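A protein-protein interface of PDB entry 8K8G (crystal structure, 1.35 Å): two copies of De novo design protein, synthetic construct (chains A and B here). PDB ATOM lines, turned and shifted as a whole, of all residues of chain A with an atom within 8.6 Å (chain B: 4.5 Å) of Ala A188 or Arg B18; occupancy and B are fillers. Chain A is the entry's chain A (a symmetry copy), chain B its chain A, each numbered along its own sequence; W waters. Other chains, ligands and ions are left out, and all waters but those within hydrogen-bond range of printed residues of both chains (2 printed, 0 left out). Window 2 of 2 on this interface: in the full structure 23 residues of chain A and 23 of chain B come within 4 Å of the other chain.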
ATOM      1  N   PRO A  30     -15.067 -29.752 -27.267  1.00  0.00           N
ATOM      2  CA  PRO A  30     -15.592 -29.698 -25.901  1.00  0.00           C
ATOM      3  C   PRO A  30     -14.839 -30.634 -24.973  1.00  0.00           C
ATOM      4  O   PRO A  30     -14.322 -31.671 -25.383  1.00  0.00           O
ATOM      5  CB  PRO A  30     -17.035 -30.185 -26.074  1.00  0.00           C
ATOM      6  CG  PRO A  30     -16.959 -31.138 -27.280  1.00  0.00           C
ATOM      7  CD  PRO A  30     -15.909 -30.542 -28.183  1.00  0.00           C
ATOM      8  N   VAL A  31     -14.815 -30.270 -23.693  1.00  0.00           N
ATOM      9  CA  VAL A  31     -14.408 -31.223 -22.666  1.00  0.00           C
ATOM     10  C   VAL A  31     -15.509 -32.270 -22.531  1.00  0.00           C
ATOM     11  O   VAL A  31     -16.665 -31.936 -22.245  1.00  0.00           O
ATOM     12  CB  VAL A  31     -14.164 -30.512 -21.330  1.00  0.00           C
ATOM     13  CG1 VAL A  31     -13.860 -31.524 -20.219  1.00  0.00           C
ATOM     14  CG2 VAL A  31     -13.053 -29.487 -21.448  1.00  0.00           C
ATOM     15  N   SER A 126     -10.897 -21.795 -18.845  1.00  0.00           N
ATOM     16  CA  SER A 126     -11.226 -22.380 -17.558  1.00  0.00           C
ATOM     17  C   SER A 126     -10.162 -23.404 -17.175  1.00  0.00           C
ATOM     18  O   SER A 126      -9.491 -23.969 -18.045  1.00  0.00           O
ATOM     19  CB  SER A 126     -12.581 -23.068 -17.636  1.00  0.00           C
ATOM     20  OG  SER A 126     -12.522 -24.188 -18.521  1.00  0.00           O
ATOM     21  N   GLY A 185     -13.200 -26.062 -24.562  1.00  0.00           N
ATOM     22  CA  GLY A 185     -14.108 -25.445 -23.617  1.00  0.00           C
ATOM     23  C   GLY A 185     -14.922 -26.445 -22.839  1.00  0.00           C
ATOM     24  O   GLY A 185     -15.395 -27.452 -23.384  1.00  0.00           O
ATOM     25  N   ASP A 186     -15.084 -26.166 -21.548  1.00  0.00           N
ATOM     26  CA  ASP A 186     -16.074 -26.879 -20.755  1.00  0.00           C
ATOM     27  C   ASP A 186     -17.463 -26.493 -21.268  1.00  0.00           C
ATOM     28  O   ASP A 186     -17.770 -25.294 -21.361  1.00  0.00           O
ATOM     29  CB  ASP A 186     -15.917 -26.476 -19.289  1.00  0.00           C
ATOM     30  CG  ASP A 186     -16.916 -27.170 -18.407  1.00  0.00           C
ATOM     31  OD1 ASP A 186     -18.115 -26.889 -18.568  1.00  0.00           O
ATOM     32  OD2 ASP A 186     -16.498 -28.022 -17.599  1.00  0.00           O
ATOM     33  N   PRO A 187     -18.326 -27.461 -21.602  1.00  0.00           N
ATOM     34  CA  PRO A 187     -19.577 -27.123 -22.321  1.00  0.00           C
ATOM     35  C   PRO A 187     -20.498 -26.161 -21.601  1.00  0.00           C
ATOM     36  O   PRO A 187     -21.331 -25.514 -22.250  1.00  0.00           O
ATOM     37  CB  PRO A 187     -20.249 -28.488 -22.526  1.00  0.00           C
ATOM     38  CG  PRO A 187     -19.099 -29.435 -22.618  1.00  0.00           C
ATOM     39  CD  PRO A 187     -18.071 -28.912 -21.620  1.00  0.00           C
ATOM     40  N   ALA A 188     -20.383 -26.040 -20.291  1.00  0.00           N
ATOM     41  CA  ALA A 188     -21.280 -25.203 -19.514  1.00  0.00           C
ATOM     42  C   ALA A 188     -20.708 -23.834 -19.177  1.00  0.00           C
ATOM     43  O   ALA A 188     -21.431 -22.994 -18.630  1.00  0.00           O
ATOM     44  CB  ALA A 188     -21.612 -25.921 -18.213  1.00  0.00           C
ATOM     45  N   ASN A 189     -19.441 -23.589 -19.486  1.00  0.00           N
ATOM     46  CA  ASN A 189     -18.724 -22.436 -18.958  1.00  0.00           C
ATOM     47  C   ASN A 189     -18.924 -21.266 -19.913  1.00  0.00           C
ATOM     48  O   ASN A 189     -18.478 -21.340 -21.063  1.00  0.00           O
ATOM     49  CB  ASN A 189     -17.244 -22.783 -18.834  1.00  0.00           C
ATOM     50  CG  ASN A 189     -16.419 -21.667 -18.222  1.00  0.00           C
ATOM     51  OD1 ASN A 189     -16.415 -20.542 -18.697  1.00  0.00           O
ATOM     52  ND2 ASN A 189     -15.711 -21.989 -17.160  1.00  0.00           N
ATOM     53  N   PRO A 190     -19.595 -20.187 -19.496  1.00  0.00           N
ATOM     54  CA  PRO A 190     -19.812 -19.070 -20.422  1.00  0.00           C
ATOM     55  C   PRO A 190     -18.531 -18.372 -20.811  1.00  0.00           C
ATOM     56  O   PRO A 190     -18.464 -17.815 -21.910  1.00  0.00           O
ATOM     57  CB  PRO A 190     -20.738 -18.129 -19.640  1.00  0.00           C
ATOM     58  CG  PRO A 190     -20.544 -18.495 -18.244  1.00  0.00           C
ATOM     59  CD  PRO A 190     -20.232 -19.956 -18.196  1.00  0.00           C
ATOM     60  N   THR A 191     -17.528 -18.352 -19.923  1.00  0.00           N
ATOM     61  CA  THR A 191     -16.240 -17.762 -20.281  1.00  0.00           C
ATOM     62  C   THR A 191     -15.587 -18.537 -21.416  1.00  0.00           C
ATOM     63  O   THR A 191     -15.130 -17.946 -22.399  1.00  0.00           O
ATOM     64  CB  THR A 191     -15.313 -17.686 -19.064  1.00  0.00           C
ATOM     65  OG1 THR A 191     -15.965 -16.982 -18.001  1.00  0.00           O
ATOM     66  CG2 THR A 191     -14.023 -16.954 -19.415  1.00  0.00           C
ATOM     67  N   ASP A 192     -15.536 -19.869 -21.302  1.00  0.00           N
ATOM     68  CA  ASP A 192     -15.019 -20.668 -22.411  1.00  0.00           C
ATOM     69  C   ASP A 192     -15.809 -20.416 -23.693  1.00  0.00           C
ATOM     70  O   ASP A 192     -15.222 -20.282 -24.773  1.00  0.00           O
ATOM     71  CB  ASP A 192     -15.036 -22.163 -22.086  1.00  0.00           C
ATOM     72  CG  ASP A 192     -13.967 -22.576 -21.084  1.00  0.00           C
ATOM     73  OD1 ASP A 192     -12.993 -21.826 -20.892  1.00  0.00           O
ATOM     74  OD2 ASP A 192     -14.078 -23.688 -20.541  1.00  0.00           O
ATOM     75  N   ALA A 193     -17.138 -20.346 -23.594  1.00  0.00           N
ATOM     76  CA  ALA A 193     -17.951 -20.101 -24.781  1.00  0.00           C
ATOM     77  C   ALA A 193     -17.683 -18.719 -25.360  1.00  0.00           C
ATOM     78  O   ALA A 193     -17.636 -18.547 -26.585  1.00  0.00           O
ATOM     79  CB  ALA A 193     -19.430 -20.273 -24.450  1.00  0.00           C
ATOM     80  N   LEU B  14     -30.899 -24.284 -27.252  1.00  0.00           N
ATOM     81  CA  LEU B  14     -29.759 -24.718 -26.445  1.00  0.00           C
ATOM     82  C   LEU B  14     -30.085 -24.623 -24.963  1.00  0.00           C
ATOM     83  O   LEU B  14     -29.818 -25.547 -24.185  1.00  0.00           O
ATOM     84  CB  LEU B  14     -28.551 -23.844 -26.763  1.00  0.00           C
ATOM     85  CG  LEU B  14     -27.921 -24.025 -28.139  1.00  0.00           C
ATOM     86  CD1 LEU B  14     -26.933 -22.901 -28.395  1.00  0.00           C
ATOM     87  CD2 LEU B  14     -27.219 -25.390 -28.244  1.00  0.00           C
ATOM     88  N   ARG B  15     -30.663 -23.496 -24.552  1.00  0.00           N
ATOM     89  CA  ARG B  15     -31.058 -23.319 -23.159  1.00  0.00           C
ATOM     90  C   ARG B  15     -32.067 -24.380 -22.747  1.00  0.00           C
ATOM     91  O   ARG B  15     -31.968 -24.957 -21.656  1.00  0.00           O
ATOM     92  CB  ARG B  15     -31.676 -21.936 -23.018  1.00  0.00           C
ATOM     93  CG  ARG B  15     -30.691 -20.878 -22.687  1.00  0.00           C
ATOM     94  CD  ARG B  15     -31.417 -19.626 -22.260  1.00  0.00           C
ATOM     95  NE  ARG B  15     -30.496 -18.504 -22.164  1.00  0.00           N
ATOM     96  CZ  ARG B  15     -29.691 -18.310 -21.130  1.00  0.00           C
ATOM     97  NH1 ARG B  15     -29.688 -19.135 -20.094  1.00  0.00           N
ATOM     98  NH2 ARG B  15     -28.863 -17.269 -21.136  1.00  0.00           N
ATOM     99  N   ALA B  16     -33.039 -24.663 -23.614  1.00  0.00           N
ATOM    100  CA  ALA B  16     -34.079 -25.620 -23.266  1.00  0.00           C
ATOM    101  C   ALA B  16     -33.527 -27.034 -23.167  1.00  0.00           C
ATOM    102  O   ALA B  16     -33.961 -27.816 -22.317  1.00  0.00           O
ATOM    103  CB  ALA B  16     -35.218 -25.547 -24.283  1.00  0.00           C
ATOM    104  N   PHE B  17     -32.577 -27.396 -24.032  1.00  0.00           N
ATOM    105  CA  PHE B  17     -32.005 -28.733 -23.932  1.00  0.00           C
ATOM    106  C   PHE B  17     -31.298 -28.931 -22.602  1.00  0.00           C
ATOM    107  O   PHE B  17     -31.436 -29.983 -21.967  1.00  0.00           O
ATOM    108  CB  PHE B  17     -31.062 -29.008 -25.111  1.00  0.00           C
ATOM    109  CG  PHE B  17     -30.650 -30.458 -25.232  1.00  0.00           C
ATOM    110  CD1 PHE B  17     -29.569 -30.951 -24.520  1.00  0.00           C
ATOM    111  CD2 PHE B  17     -31.375 -31.332 -26.036  1.00  0.00           C
ATOM    112  CE1 PHE B  17     -29.198 -32.287 -24.627  1.00  0.00           C
ATOM    113  CE2 PHE B  17     -31.019 -32.667 -26.143  1.00  0.00           C
ATOM    114  CZ  PHE B  17     -29.934 -33.150 -25.428  1.00  0.00           C
ATOM    115  N   ARG B  18     -30.529 -27.931 -22.179  1.00  0.00           N
ATOM    116  CA  ARG B  18     -29.826 -28.013 -20.906  1.00  0.00           C
ATOM    117  C   ARG B  18     -30.794 -28.010 -19.723  1.00  0.00           C
ATOM    118  O   ARG B  18     -30.582 -28.728 -18.734  1.00  0.00           O
ATOM    119  CB  ARG B  18     -28.824 -26.861 -20.790  1.00  0.00           C
ATOM    120  CG  ARG B  18     -27.613 -27.000 -21.708  1.00  0.00           C
ATOM    121  CD  ARG B  18     -26.557 -25.904 -21.494  1.00  0.00           C
ATOM    122  NE  ARG B  18     -26.066 -25.828 -20.124  1.00  0.00           N
ATOM    123  CZ  ARG B  18     -25.201 -26.665 -19.569  1.00  0.00           C
ATOM    124  NH1 ARG B  18     -24.654 -27.655 -20.253  1.00  0.00           N
ATOM    125  NH2 ARG B  18     -24.894 -26.519 -18.285  1.00  0.00           N
ATOM    126  N   ALA B  19     -31.858 -27.198 -19.791  1.00  0.00           N
ATOM    127  CA  ALA B  19     -32.834 -27.164 -18.704  1.00  0.00           C
ATOM    128  C   ALA B  19     -33.552 -28.495 -18.563  1.00  0.00           C
ATOM    129  O   ALA B  19     -34.023 -28.834 -17.470  1.00  0.00           O
ATOM    130  CB  ALA B  19     -33.848 -26.044 -18.938  1.00  0.00           C
ATOM    131  N   ALA B  20     -33.664 -29.256 -19.652  1.00  0.00           N
ATOM    132  CA  ALA B  20     -34.279 -30.575 -19.582  1.00  0.00           C
ATOM    133  C   ALA B  20     -33.336 -31.650 -19.056  1.00  0.00           C
ATOM    134  O   ALA B  20     -33.774 -32.785 -18.842  1.00  0.00           O
ATOM    135  CB  ALA B  20     -34.876 -30.974 -20.931  1.00  0.00           C
ATOM    136  N   GLY B  21     -32.064 -31.331 -18.832  1.00  0.00           N
ATOM    137  CA  GLY B  21     -31.160 -32.257 -18.196  1.00  0.00           C
ATOM    138  C   GLY B  21     -30.042 -32.815 -19.048  1.00  0.00           C
ATOM    139  O   GLY B  21     -29.346 -33.731 -18.593  1.00  0.00           O
ATOM    140  N   GLY B  22     -29.824 -32.298 -20.251  1.00  0.00           N
ATOM    141  CA  GLY B  22     -28.788 -32.807 -21.123  1.00  0.00           C
ATOM    142  C   GLY B  22     -27.741 -31.759 -21.446  1.00  0.00           C
ATOM    143  O   GLY B  22     -28.034 -30.565 -21.513  1.00  0.00           O
ATOM    144  N   THR B  23     -26.519 -32.222 -21.664  1.00  0.00           N
ATOM    145  CA  THR B  23     -25.434 -31.349 -22.102  1.00  0.00           C
ATOM    146  C   THR B  23     -25.450 -31.219 -23.627  1.00  0.00           C
ATOM    147  O   THR B  23     -25.632 -32.206 -24.343  1.00  0.00           O
ATOM    148  CB  THR B  23     -24.099 -31.950 -21.663  1.00  0.00           C
ATOM    149  OG1 THR B  23     -24.037 -31.934 -20.244  1.00  0.00           O
ATOM    150  CG2 THR B  23     -22.916 -31.157 -22.230  1.00  0.00           C
ATOM    151  N   VAL B  24     -25.265 -29.995 -24.130  1.00  0.00           N
ATOM    152  CA  VAL B  24     -24.966 -29.780 -25.546  1.00  0.00           C
ATOM    153  C   VAL B  24     -23.454 -29.739 -25.725  1.00  0.00           C
ATOM    154  O   VAL B  24     -22.771 -28.905 -25.123  1.00  0.00           O
ATOM    155  CB  VAL B  24     -25.605 -28.500 -26.106  1.00  0.00           C
ATOM    156  CG1 VAL B  24     -25.282 -28.387 -27.612  1.00  0.00           C
ATOM    157  CG2 VAL B  24     -27.111 -28.481 -25.868  1.00  0.00           C
ATOM    158  N   LEU B 207     -25.398 -19.742 -22.540  1.00  0.00           N
ATOM    159  CA  LEU B 207     -24.728 -20.112 -21.300  1.00  0.00           C
ATOM    160  C   LEU B 207     -24.635 -18.965 -20.309  1.00  0.00           C
ATOM    161  O   LEU B 207     -24.253 -19.194 -19.157  1.00  0.00           O
ATOM    162  CB  LEU B 207     -23.317 -20.608 -21.620  1.00  0.00           C
ATOM    163  CG  LEU B 207     -23.222 -21.886 -22.450  1.00  0.00           C
ATOM    164  CD1 LEU B 207     -21.767 -22.308 -22.558  1.00  0.00           C
ATOM    165  CD2 LEU B 207     -24.085 -23.007 -21.871  1.00  0.00           C
HETATM  166  O   HOH W   1     -23.880 -27.403 -22.965  1.00  0.00           O
HETATM  167  O   HOH W   2     -23.937 -21.934 -18.277  1.00  0.00           O
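Hydrophobic or aromatic side chains of chain B that line the printed part of chain A: Leu B207.
Printed residues of chain B within 4 Å of Pro A187: Thr B23 (3.8 Å), Val B24 (3.6 Å) and Leu B207 (3.3 Å).
Of chain B, only Arg B18 and Leu B207 come within 4 Å of Ala A188.
Arg B18 touches one residue of chain A.
Printed residues of chain A within 4 Å of Leu B207: Pro A187 (3.3 Å), Ala A188 (3.9 Å), Asn A189 (3.7 Å), Pro A190 (3.7 Å) and Ala A193 (3.6 Å).
The nearest residue of chain A that does not touch Arg B18 is Pro A187 (4.4 Å).
The nearest printed residue of chain B that does not touch Ala A193 is Leu B14 (8.9 Å).
No position is printed for both chains.
Of the 8 pairs that touch across the chains among the printed residues, none has its exchanged pair printed and touching as well.
Water W2 lies within hydrogen-bond range of O of Ala A188 and O of Leu B207.
Water W1 lies within hydrogen-bond range of NH1 of Arg B18, O of Val B24 and O of Pro A187.
Among the printed residues, pairs that only touch across the chains: Pro A187 with Leu B207, Ala A188 with Arg B18, Ala A193 with Leu B207, Pro A187 with Val B24, Pro A190 with Leu B207, Asn A189 with Leu B207, Pro A187 with Thr B23 and Ala A188 with Leu B207.
OD1 of Asp A186 sits at hydrogen-bond distance from N of Ala A188 (3.0 Å).
The side-chain amide oxygen (OD1) of Asn A189 is in hydrogen-bond range of the backbone NH (N) of Thr A191.
The backbone NH (N) of Asp A192 sits at hydrogen-bond distance from the side-chain amide oxygen (OD1) of Asn A189 (2.8 Å).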
